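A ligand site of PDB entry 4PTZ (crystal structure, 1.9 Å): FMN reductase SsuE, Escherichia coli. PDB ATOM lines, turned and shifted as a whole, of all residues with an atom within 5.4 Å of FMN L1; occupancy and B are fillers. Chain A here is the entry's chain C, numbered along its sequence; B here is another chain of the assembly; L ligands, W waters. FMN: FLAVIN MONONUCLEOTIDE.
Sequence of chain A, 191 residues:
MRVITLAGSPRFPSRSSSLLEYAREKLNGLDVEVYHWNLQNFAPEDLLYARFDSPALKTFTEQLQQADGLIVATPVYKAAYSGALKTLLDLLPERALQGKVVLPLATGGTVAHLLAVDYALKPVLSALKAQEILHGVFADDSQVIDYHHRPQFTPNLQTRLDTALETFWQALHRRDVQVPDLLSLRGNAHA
Residues that only touch FMN L1: Asp 90 of chain B (3.2 Å), Tyr 77 (3.3 Å), Pro 75 (3.3 Å), Gly 108 (3.5 Å) and Phe 52 of chain B (3.9 Å). Hydrophobic or aromatic side chains within 4 Å of FMN L1: Pro 75, Val 76, Tyr 77, His 113 and Phe 52 of chain B. The nearest printed residue that does not touch FMN L1 is Ser 17 (4.2 Å).
O2' of FMN L2 lies close to O3' of FMN L1 (3.5 Å).
The side-chain carboxylate of Asp 141 is in salt-bridge range of the guanidinium group of Arg 15. OG of Ser 14 is in hydrogen-bond range of OG of Ser 16, 3.3 Å away. The backbone carbonyl oxygen of Thr 74 lies within hydrogen-bond range of the backbone NH of Thr 107 (3.1 Å). N of Asp 141 lies within hydrogen-bond range of O of Gly 108 (2.8 Å). The side-chain hydroxyl of Ser 9 is in hydrogen-bond range of the backbone NH of Arg 11 (3.1 Å). OG of Ser 14 sits at hydrogen-bond distance from N of Ser 17 (2.8 Å). The guanidinium group (NH2) of Arg 11 sits at hydrogen-bond distance from the side-chain hydroxyl (OH) of Tyr 147 (3.1 Å). The backbone NH (N) of Val 76 lies within hydrogen-bond range of the backbone carbonyl oxygen (O) of Thr 107, at 2.9 Å.
Water W2 lies within hydrogen-bond range of O2P of FMN L1 (2.5 Å), OH of Tyr 77 (2.6 Å) and NE of Arg 11 (3.3 Å). Water W1 bridges O3' of FMN L1 (2.7 Å) and O3' of FMN L2 (3.0 Å).
The guanidinium group (NH1) of Arg 15 sits at hydrogen-bond distance from an oxygen (O4') of FMN L1 (3.0 Å). The side-chain hydroxyl (OG) of Ser 16 lies within hydrogen-bond range of an oxygen (O3P) of FMN L1 (2.6 Å). NH2 of Arg 11 lies within salt-bridge range of O1P of FMN L1, 2.9 Å away. The backbone NH (N) of Val 76 is in hydrogen-bond range of an oxygen (O2') of FMN L1. The side-chain amino group (NZ) of Lys 78 sits at hydrogen-bond distance from an oxygen (O4) of FMN L2 (2.6 Å). An oxygen (O3P) of FMN L1 sits at hydrogen-bond distance from the backbone NH (N) of Ser 16 (2.8 Å). OG1 of Thr 107 lies within hydrogen-bond range of O4' of FMN L1, at 2.8 Å. The backbone NH (N) of Lys 78 lies within hydrogen-bond range of an oxygen (O4) of FMN L1. The side-chain carboxylate (OD1) of Asp 141 lies within hydrogen-bond range of an oxygen (O4') of FMN L1. An oxygen (O2) of FMN L1 is in hydrogen-bond range of the backbone NH (N) of Thr 110. O of Val 76 is in hydrogen-bond range of O2' of FMN L1, at 2.7 Å. NH1 of Arg 11 lies within salt-bridge range of O1P of FMN L2 (2.8 Å). N of Ala 79 lies within hydrogen-bond range of O4 of FMN L1, at 3.1 Å. O2P of FMN L2 lies within salt-bridge range of NH1 of Arg 15 (3.2 Å). The backbone carbonyl oxygen (O) of Thr 107 sits at hydrogen-bond distance from an oxygen (O2') of FMN L1. The backbone NH (N) of Arg 15 is in hydrogen-bond range of an oxygen (O1P) of FMN L1 (2.7 Å). The backbone NH (N) of Gly 109 lies within hydrogen-bond range of an oxygen (O2) of FMN L1, 3.0 Å away. A nitrogen (N3) of FMN L1 is in hydrogen-bond range of a ring nitrogen (ND1) of His 113, at 2.9 Å. The side-chain hydroxyl (OH) of Tyr 147 lies within hydrogen-bond range of an oxygen (O3P) of FMN L2 (3.3 Å). The side-chain hydroxyl (OG) of Ser 14 is in hydrogen-bond range of an oxygen (O3P) of FMN L1, 2.6 Å away. The side-chain hydroxyl (OG) of Ser 9 sits at hydrogen-bond distance from an oxygen (O2P) of FMN L1 (2.6 Å).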
ATOM      1  N   SER A   9      -0.079  10.082  22.414  1.00  0.00           N
ATOM      2  CA  SER A   9      -1.319  10.047  21.649  1.00  0.00           C
ATOM      3  C   SER A   9      -1.088  10.414  20.184  1.00  0.00           C
ATOM      4  O   SER A   9      -0.338  11.343  19.877  1.00  0.00           O
ATOM      5  CB  SER A   9      -2.362  10.984  22.232  1.00  0.00           C
ATOM      6  OG  SER A   9      -3.438  10.970  21.330  1.00  0.00           O
ATOM      7  N   PRO A  10      -1.759   9.730  19.267  1.00  0.00           N
ATOM      8  CA  PRO A  10      -1.704  10.115  17.857  1.00  0.00           C
ATOM      9  C   PRO A  10      -2.620  11.243  17.459  1.00  0.00           C
ATOM     10  O   PRO A  10      -2.566  11.675  16.314  1.00  0.00           O
ATOM     11  CB  PRO A  10      -2.148   8.851  17.131  1.00  0.00           C
ATOM     12  CG  PRO A  10      -3.108   8.224  18.056  1.00  0.00           C
ATOM     13  CD  PRO A  10      -2.533   8.484  19.457  1.00  0.00           C
ATOM     14  N   ARG A  11      -3.475  11.687  18.355  1.00  0.00           N
ATOM     15  CA  ARG A  11      -4.395  12.744  17.996  1.00  0.00           C
ATOM     16  C   ARG A  11      -4.076  14.036  18.669  1.00  0.00           C
ATOM     17  O   ARG A  11      -3.369  14.100  19.674  1.00  0.00           O
ATOM     18  CB  ARG A  11      -5.837  12.339  18.247  1.00  0.00           C
ATOM     19  CG  ARG A  11      -6.150  11.954  19.621  1.00  0.00           C
ATOM     20  CD  ARG A  11      -7.659  11.671  19.729  1.00  0.00           C
ATOM     21  NE  ARG A  11      -8.057  11.873  21.120  1.00  0.00           N
ATOM     22  CZ  ARG A  11      -9.294  12.078  21.523  1.00  0.00           C
ATOM     23  NH1 ARG A  11     -10.303  12.114  20.658  1.00  0.00           N
ATOM     24  NH2 ARG A  11      -9.494  12.252  22.820  1.00  0.00           N
ATOM     25  N   PRO A  13      -6.170  17.822  19.375  1.00  0.00           N
ATOM     26  CA  PRO A  13      -5.720  17.777  20.785  1.00  0.00           C
ATOM     27  C   PRO A  13      -5.894  16.411  21.453  1.00  0.00           C
ATOM     28  O   PRO A  13      -6.753  15.621  21.055  1.00  0.00           O
ATOM     29  CB  PRO A  13      -6.629  18.795  21.456  1.00  0.00           C
ATOM     30  CG  PRO A  13      -7.787  18.913  20.581  1.00  0.00           C
ATOM     31  CD  PRO A  13      -7.299  18.741  19.205  1.00  0.00           C
ATOM     32  N   SER A  14      -5.103  16.159  22.481  1.00  0.00           N
ATOM     33  CA  SER A  14      -5.046  14.877  23.163  1.00  0.00           C
ATOM     34  C   SER A  14      -5.382  15.061  24.644  1.00  0.00           C
ATOM     35  O   SER A  14      -4.924  15.997  25.272  1.00  0.00           O
ATOM     36  CB  SER A  14      -3.652  14.282  22.981  1.00  0.00           C
ATOM     37  OG  SER A  14      -3.244  13.507  24.084  1.00  0.00           O
ATOM     38  N   ARG A  15      -6.202  14.181  25.188  1.00  0.00           N
ATOM     39  CA  ARG A  15      -6.506  14.178  26.613  1.00  0.00           C
ATOM     40  C   ARG A  15      -5.266  13.844  27.443  1.00  0.00           C
ATOM     41  O   ARG A  15      -4.970  14.564  28.407  1.00  0.00           O
ATOM     42  CB  ARG A  15      -7.634  13.200  26.878  1.00  0.00           C
ATOM     43  CG  ARG A  15      -8.190  13.278  28.212  1.00  0.00           C
ATOM     44  CD  ARG A  15      -9.237  12.243  28.460  1.00  0.00           C
ATOM     45  NE  ARG A  15     -10.567  12.595  27.976  1.00  0.00           N
ATOM     46  CZ  ARG A  15     -11.065  12.180  26.829  1.00  0.00           C
ATOM     47  NH1 ARG A  15     -10.340  11.442  25.998  1.00  0.00           N
ATOM     48  NH2 ARG A  15     -12.266  12.508  26.485  1.00  0.00           N
ATOM     49  N   SER A  16      -4.537  12.785  27.109  1.00  0.00           N
ATOM     50  CA  SER A  16      -3.332  12.458  27.869  1.00  0.00           C
ATOM     51  C   SER A  16      -2.296  13.569  27.762  1.00  0.00           C
ATOM     52  O   SER A  16      -1.553  13.826  28.726  1.00  0.00           O
ATOM     53  CB  SER A  16      -2.734  11.067  27.492  1.00  0.00           C
ATOM     54  OG  SER A  16      -2.414  10.999  26.107  1.00  0.00           O
ATOM     55  N   SER A  17      -2.210  14.247  26.620  1.00  0.00           N
ATOM     56  CA  SER A  17      -1.285  15.402  26.530  1.00  0.00           C
ATOM     57  C   SER A  17      -1.633  16.564  27.462  1.00  0.00           C
ATOM     58  O   SER A  17      -0.744  17.356  27.745  1.00  0.00           O
ATOM     59  CB  SER A  17      -1.127  15.922  25.119  1.00  0.00           C
ATOM     60  OG  SER A  17      -0.428  14.942  24.334  1.00  0.00           O
ATOM     61  N   THR A  74       0.257   8.458  27.606  1.00  0.00           N
ATOM     62  CA  THR A  74      -0.358   7.635  26.596  1.00  0.00           C
ATOM     63  C   THR A  74      -1.876   7.514  26.840  1.00  0.00           C
ATOM     64  O   THR A  74      -2.315   7.557  27.973  1.00  0.00           O
ATOM     65  CB  THR A  74       0.338   6.215  26.482  1.00  0.00           C
ATOM     66  OG1 THR A  74      -0.231   5.492  25.408  1.00  0.00           O
ATOM     67  CG2 THR A  74       0.179   5.417  27.755  1.00  0.00           C
ATOM     68  N   PRO A  75      -2.667   7.413  25.756  1.00  0.00           N
ATOM     69  CA  PRO A  75      -4.028   6.850  25.868  1.00  0.00           C
ATOM     70  C   PRO A  75      -3.886   5.340  26.108  1.00  0.00           C
ATOM     71  O   PRO A  75      -2.823   4.794  25.806  1.00  0.00           O
ATOM     72  CB  PRO A  75      -4.609   7.131  24.486  1.00  0.00           C
ATOM     73  CG  PRO A  75      -3.457   7.065  23.571  1.00  0.00           C
ATOM     74  CD  PRO A  75      -2.323   7.705  24.361  1.00  0.00           C
ATOM     75  N   VAL A  76      -4.905   4.716  26.663  1.00  0.00           N
ATOM     76  CA  VAL A  76      -5.023   3.278  26.675  1.00  0.00           C
ATOM     77  C   VAL A  76      -5.676   2.868  25.339  1.00  0.00           C
ATOM     78  O   VAL A  76      -6.820   3.255  25.037  1.00  0.00           O
ATOM     79  CB  VAL A  76      -5.902   2.767  27.835  1.00  0.00           C
ATOM     80  CG1 VAL A  76      -5.998   1.225  27.808  1.00  0.00           C
ATOM     81  CG2 VAL A  76      -5.320   3.204  29.181  1.00  0.00           C
ATOM     82  N   TYR A  77      -4.944   2.118  24.548  1.00  0.00           N
ATOM     83  CA  TYR A  77      -5.477   1.553  23.317  1.00  0.00           C
ATOM     84  C   TYR A  77      -5.417   0.025  23.466  1.00  0.00           C
ATOM     85  O   TYR A  77      -4.327  -0.551  23.669  1.00  0.00           O
ATOM     86  CB  TYR A  77      -4.638   1.989  22.141  1.00  0.00           C
ATOM     87  CG  TYR A  77      -4.873   3.383  21.571  1.00  0.00           C
ATOM     88  CD1 TYR A  77      -5.803   4.264  22.119  1.00  0.00           C
ATOM     89  CD2 TYR A  77      -4.188   3.781  20.429  1.00  0.00           C
ATOM     90  CE1 TYR A  77      -6.013   5.542  21.585  1.00  0.00           C
ATOM     91  CE2 TYR A  77      -4.386   5.069  19.879  1.00  0.00           C
ATOM     92  CZ  TYR A  77      -5.319   5.920  20.455  1.00  0.00           C
ATOM     93  OH  TYR A  77      -5.496   7.143  19.879  1.00  0.00           O
ATOM     94  N   LYS A  78      -6.572  -0.632  23.385  1.00  0.00           N
ATOM     95  CA  LYS A  78      -6.638  -2.105  23.474  1.00  0.00           C
ATOM     96  C   LYS A  78      -5.918  -2.634  24.714  1.00  0.00           C
ATOM     97  O   LYS A  78      -5.096  -3.517  24.617  1.00  0.00           O
ATOM     98  CB  LYS A  78      -6.073  -2.789  22.188  1.00  0.00           C
ATOM     99  CG  LYS A  78      -6.563  -2.225  20.850  1.00  0.00           C
ATOM    100  CD  LYS A  78      -8.021  -2.378  20.618  1.00  0.00           C
ATOM    101  CE  LYS A  78      -8.464  -1.657  19.335  1.00  0.00           C
ATOM    102  NZ  LYS A  78      -9.898  -1.767  19.073  1.00  0.00           N
ATOM    103  N   ALA A  79      -6.212  -2.043  25.885  1.00  0.00           N
ATOM    104  CA  ALA A  79      -5.685  -2.506  27.158  1.00  0.00           C
ATOM    105  C   ALA A  79      -4.155  -2.409  27.351  1.00  0.00           C
ATOM    106  O   ALA A  79      -3.602  -3.136  28.178  1.00  0.00           O
ATOM    107  CB  ALA A  79      -6.179  -3.934  27.450  1.00  0.00           C
ATOM    108  N   THR A 107      -4.387   8.068  30.194  1.00  0.00           N
ATOM    109  CA  THR A 107      -5.828   8.227  30.277  1.00  0.00           C
ATOM    110  C   THR A 107      -6.517   7.143  29.511  1.00  0.00           C
ATOM    111  O   THR A 107      -6.052   6.731  28.480  1.00  0.00           O
ATOM    112  CB  THR A 107      -6.302   9.582  29.791  1.00  0.00           C
ATOM    113  OG1 THR A 107      -5.921   9.764  28.426  1.00  0.00           O
ATOM    114  CG2 THR A 107      -5.782  10.733  30.666  1.00  0.00           C
ATOM    115  N   GLY A 108      -7.671   6.695  30.022  1.00  0.00           N
ATOM    116  CA  GLY A 108      -8.367   5.566  29.440  1.00  0.00           C
ATOM    117  C   GLY A 108      -9.857   5.826  29.415  1.00  0.00           C
ATOM    118  O   GLY A 108     -10.393   6.591  30.270  1.00  0.00           O
ATOM    119  N   GLY A 109     -10.534   5.219  28.451  1.00  0.00           N
ATOM    120  CA  GLY A 109     -11.966   5.385  28.315  1.00  0.00           C
ATOM    121  C   GLY A 109     -12.734   4.758  29.460  1.00  0.00           C
ATOM    122  O   GLY A 109     -13.823   5.214  29.809  1.00  0.00           O
ATOM    123  N   THR A 110     -12.209   3.648  29.974  1.00  0.00           N
ATOM    124  CA  THR A 110     -12.825   2.996  31.094  1.00  0.00           C
ATOM    125  C   THR A 110     -11.843   2.811  32.253  1.00  0.00           C
ATOM    126  O   THR A 110     -10.697   2.470  32.064  1.00  0.00           O
ATOM    127  CB  THR A 110     -13.402   1.608  30.728  1.00  0.00           C
ATOM    128  OG1 THR A 110     -13.864   1.007  31.929  1.00  0.00           O
ATOM    129  CG2 THR A 110     -12.331   0.677  30.044  1.00  0.00           C
ATOM    130  N   HIS A 113      -9.499  -0.471  32.667  1.00  0.00           N
ATOM    131  CA  HIS A 113      -8.176  -0.677  32.082  1.00  0.00           C
ATOM    132  C   HIS A 113      -7.084   0.092  32.796  1.00  0.00           C
ATOM    133  O   HIS A 113      -6.012   0.291  32.263  1.00  0.00           O
ATOM    134  CB  HIS A 113      -8.204  -0.374  30.589  1.00  0.00           C
ATOM    135  CG  HIS A 113      -8.871  -1.442  29.799  1.00  0.00           C
ATOM    136  ND1 HIS A 113      -9.044  -1.366  28.434  1.00  0.00           N
ATOM    137  CD2 HIS A 113      -9.350  -2.653  30.179  1.00  0.00           C
ATOM    138  CE1 HIS A 113      -9.633  -2.475  28.016  1.00  0.00           C
ATOM    139  NE2 HIS A 113      -9.833  -3.265  29.065  1.00  0.00           N
ATOM    140  N   ASP A 141     -11.358   8.972  31.303  1.00  0.00           N
ATOM    141  CA  ASP A 141     -11.681  10.184  30.564  1.00  0.00           C
ATOM    142  C   ASP A 141     -12.524  11.211  31.282  1.00  0.00           C
ATOM    143  O   ASP A 141     -12.361  12.412  31.066  1.00  0.00           O
ATOM    144  CB  ASP A 141     -12.409   9.774  29.280  1.00  0.00           C
ATOM    145  CG  ASP A 141     -11.495   9.206  28.265  1.00  0.00           C
ATOM    146  OD1 ASP A 141     -10.299   9.015  28.577  1.00  0.00           O
ATOM    147  OD2 ASP A 141     -11.995   8.900  27.151  1.00  0.00           O
ATOM    148  N   TYR A 147      -9.610  19.391  27.704  1.00  0.00           N
ATOM    149  CA  TYR A 147      -8.269  19.197  27.140  1.00  0.00           C
ATOM    150  C   TYR A 147      -8.146  19.964  25.821  1.00  0.00           C
ATOM    151  O   TYR A 147      -7.128  19.869  25.170  1.00  0.00           O
ATOM    152  CB  TYR A 147      -7.898  17.696  26.945  1.00  0.00           C
ATOM    153  CG  TYR A 147      -8.811  16.899  26.006  1.00  0.00           C
ATOM    154  CD1 TYR A 147     -10.019  16.385  26.447  1.00  0.00           C
ATOM    155  CD2 TYR A 147      -8.449  16.671  24.690  1.00  0.00           C
ATOM    156  CE1 TYR A 147     -10.848  15.664  25.599  1.00  0.00           C
ATOM    157  CE2 TYR A 147      -9.256  15.969  23.832  1.00  0.00           C
ATOM    158  CZ  TYR A 147     -10.466  15.468  24.292  1.00  0.00           C
ATOM    159  OH  TYR A 147     -11.265  14.760  23.443  1.00  0.00           O
ATOM    160  N   PHE B  52      -8.985   5.953  10.701  1.00  0.00           N
ATOM    161  CA  PHE B  52      -9.910   4.844  10.452  1.00  0.00           C
ATOM    162  C   PHE B  52     -10.503   4.780   9.056  1.00  0.00           C
ATOM    163  O   PHE B  52     -11.024   3.733   8.659  1.00  0.00           O
ATOM    164  CB  PHE B  52     -11.034   4.874  11.503  1.00  0.00           C
ATOM    165  CG  PHE B  52     -10.534   4.842  12.914  1.00  0.00           C
ATOM    166  CD1 PHE B  52     -10.189   3.629  13.524  1.00  0.00           C
ATOM    167  CD2 PHE B  52     -10.352   6.027  13.637  1.00  0.00           C
ATOM    168  CE1 PHE B  52      -9.709   3.608  14.822  1.00  0.00           C
ATOM    169  CE2 PHE B  52      -9.871   5.997  14.929  1.00  0.00           C
ATOM    170  CZ  PHE B  52      -9.546   4.789  15.529  1.00  0.00           C
ATOM    171  N   ASP B  90      -4.459  -1.559  16.908  1.00  0.00           N
ATOM    172  CA  ASP B  90      -5.193  -0.448  17.535  1.00  0.00           C
ATOM    173  C   ASP B  90      -6.324   0.072  16.642  1.00  0.00           C
ATOM    174  O   ASP B  90      -7.294   0.631  17.137  1.00  0.00           O
ATOM    175  CB  ASP B  90      -4.240   0.721  17.823  1.00  0.00           C
ATOM    176  CG  ASP B  90      -3.323   0.460  19.023  1.00  0.00           C
ATOM    177  OD1 ASP B  90      -3.560  -0.513  19.777  1.00  0.00           O
ATOM    178  OD2 ASP B  90      -2.367   1.252  19.218  1.00  0.00           O
ATOM    179  N   LEU B  91      -6.173  -0.083  15.328  1.00  0.00           N
ATOM    180  CA  LEU B  91      -7.167   0.391  14.348  1.00  0.00           C
ATOM    181  C   LEU B  91      -8.301  -0.583  14.094  1.00  0.00           C
ATOM    182  O   LEU B  91      -9.239  -0.246  13.377  1.00  0.00           O
ATOM    183  CB  LEU B  91      -6.456   0.632  13.004  1.00  0.00           C
ATOM    184  CG  LEU B  91      -5.661   1.948  12.931  1.00  0.00           C
ATOM    185  CD1 LEU B  91      -4.964   2.057  11.609  1.00  0.00           C
ATOM    186  CD2 LEU B  91      -6.578   3.141  13.130  1.00  0.00           C
HETATM  187  N1  FMN L   1      -9.947   3.198  26.377  1.00  0.00           N
HETATM  188  C2  FMN L   1      -9.825   2.179  27.266  1.00  0.00           C
HETATM  189  O2  FMN L   1      -9.989   2.320  28.487  1.00  0.00           O
HETATM  190  N3  FMN L   1      -9.467   0.947  26.789  1.00  0.00           N
HETATM  191  C4  FMN L   1      -9.205   0.668  25.455  1.00  0.00           C
HETATM  192  O4  FMN L   1      -8.825  -0.483  25.078  1.00  0.00           O
HETATM  193  C4A FMN L   1      -9.307   1.718  24.576  1.00  0.00           C
HETATM  194  N5  FMN L   1      -9.043   1.516  23.232  1.00  0.00           N
HETATM  195  C5A FMN L   1      -9.030   2.618  22.408  1.00  0.00           C
HETATM  196  C6  FMN L   1      -8.658   2.427  21.092  1.00  0.00           C
HETATM  197  C7  FMN L   1      -8.669   3.508  20.206  1.00  0.00           C
HETATM  198  C7M FMN L   1      -8.210   3.168  18.793  1.00  0.00           C
HETATM  199  C8  FMN L   1      -9.104   4.770  20.648  1.00  0.00           C
HETATM  200  C8M FMN L   1      -9.165   6.003  19.780  1.00  0.00           C
HETATM  201  C9  FMN L   1      -9.487   4.951  21.979  1.00  0.00           C
HETATM  202  C9A FMN L   1      -9.465   3.858  22.848  1.00  0.00           C
HETATM  203  N10 FMN L   1      -9.818   4.030  24.177  1.00  0.00           N
HETATM  204  C10 FMN L   1      -9.704   2.983  25.035  1.00  0.00           C
HETATM  205  C1' FMN L   1     -10.210   5.387  24.717  1.00  0.00           C
HETATM  206  C2' FMN L   1      -8.923   6.174  25.034  1.00  0.00           C
HETATM  207  O2' FMN L   1      -8.033   5.491  25.908  1.00  0.00           O
HETATM  208  C3' FMN L   1      -9.251   7.477  25.759  1.00  0.00           C
HETATM  209  O3' FMN L   1     -10.288   8.156  25.070  1.00  0.00           O
HETATM  210  C4' FMN L   1      -8.043   8.392  25.960  1.00  0.00           C
HETATM  211  O4' FMN L   1      -8.275   9.420  26.925  1.00  0.00           O
HETATM  212  C5' FMN L   1      -7.628   9.135  24.736  1.00  0.00           C
HETATM  213  O5' FMN L   1      -6.455   9.831  25.080  1.00  0.00           O
HETATM  214  P   FMN L   1      -5.810  10.859  24.021  1.00  0.00           P
HETATM  215  O1P FMN L   1      -6.797  11.944  23.744  1.00  0.00           O
HETATM  216  O2P FMN L   1      -5.543  10.169  22.703  1.00  0.00           O
HETATM  217  O3P FMN L   1      -4.525  11.384  24.683  1.00  0.00           O
HETATM  218  N1  FMN L   2     -12.489   3.820  19.618  1.00  0.00           N
HETATM  219  C2  FMN L   2     -11.897   3.115  18.593  1.00  0.00           C
HETATM  220  O2  FMN L   2     -11.857   3.685  17.509  1.00  0.00           O
HETATM  221  N3  FMN L   2     -11.381   1.841  18.838  1.00  0.00           N
HETATM  222  C4  FMN L   2     -11.468   1.298  20.123  1.00  0.00           C
HETATM  223  O4  FMN L   2     -11.032   0.175  20.384  1.00  0.00           O
HETATM  224  C4A FMN L   2     -12.099   2.008  21.136  1.00  0.00           C
HETATM  225  N5  FMN L   2     -12.195   1.448  22.409  1.00  0.00           N
HETATM  226  C5A FMN L   2     -12.804   2.188  23.395  1.00  0.00           C
HETATM  227  C6  FMN L   2     -12.910   1.641  24.664  1.00  0.00           C
HETATM  228  C7  FMN L   2     -13.568   2.368  25.649  1.00  0.00           C
HETATM  229  C7M FMN L   2     -13.652   1.746  27.004  1.00  0.00           C
HETATM  230  C8  FMN L   2     -14.073   3.652  25.388  1.00  0.00           C
HETATM  231  C8M FMN L   2     -14.811   4.517  26.393  1.00  0.00           C
HETATM  232  C9  FMN L   2     -13.966   4.190  24.114  1.00  0.00           C
HETATM  233  C9A FMN L   2     -13.337   3.469  23.118  1.00  0.00           C
HETATM  234  N10 FMN L   2     -13.231   4.024  21.854  1.00  0.00           N
HETATM  235  C10 FMN L   2     -12.604   3.270  20.872  1.00  0.00           C
HETATM  236  C1' FMN L   2     -13.794   5.375  21.463  1.00  0.00           C
HETATM  237  C2' FMN L   2     -12.842   6.532  21.637  1.00  0.00           C
HETATM  238  O2' FMN L   2     -12.660   6.606  23.026  1.00  0.00           O
HETATM  239  C3' FMN L   2     -13.392   7.805  20.974  1.00  0.00           C
HETATM  240  O3' FMN L   2     -12.275   8.528  20.454  1.00  0.00           O
HETATM  241  C4' FMN L   2     -14.219   8.664  21.943  1.00  0.00           C
HETATM  242  O4' FMN L   2     -15.307   7.935  22.474  1.00  0.00           O
HETATM  243  C5' FMN L   2     -14.742   9.946  21.324  1.00  0.00           C
HETATM  244  O5' FMN L   2     -14.774  10.864  22.404  1.00  0.00           O
HETATM  245  P   FMN L   2     -13.463  11.734  22.799  1.00  0.00           P
HETATM  246  O1P FMN L   2     -12.972  12.323  21.486  1.00  0.00           O
HETATM  247  O2P FMN L   2     -12.362  10.932  23.537  1.00  0.00           O
HETATM  248  O3P FMN L   2     -13.921  12.853  23.717  1.00  0.00           O
HETATM  249  O   HOH W   1     -10.045   8.532  22.417  1.00  0.00           O
HETATM  250  O   HOH W   2      -7.062   8.744  21.255  1.00  0.00           O
HETATM  251  O   HOH W   3     -10.144  -2.529  24.147  1.00  0.00           O
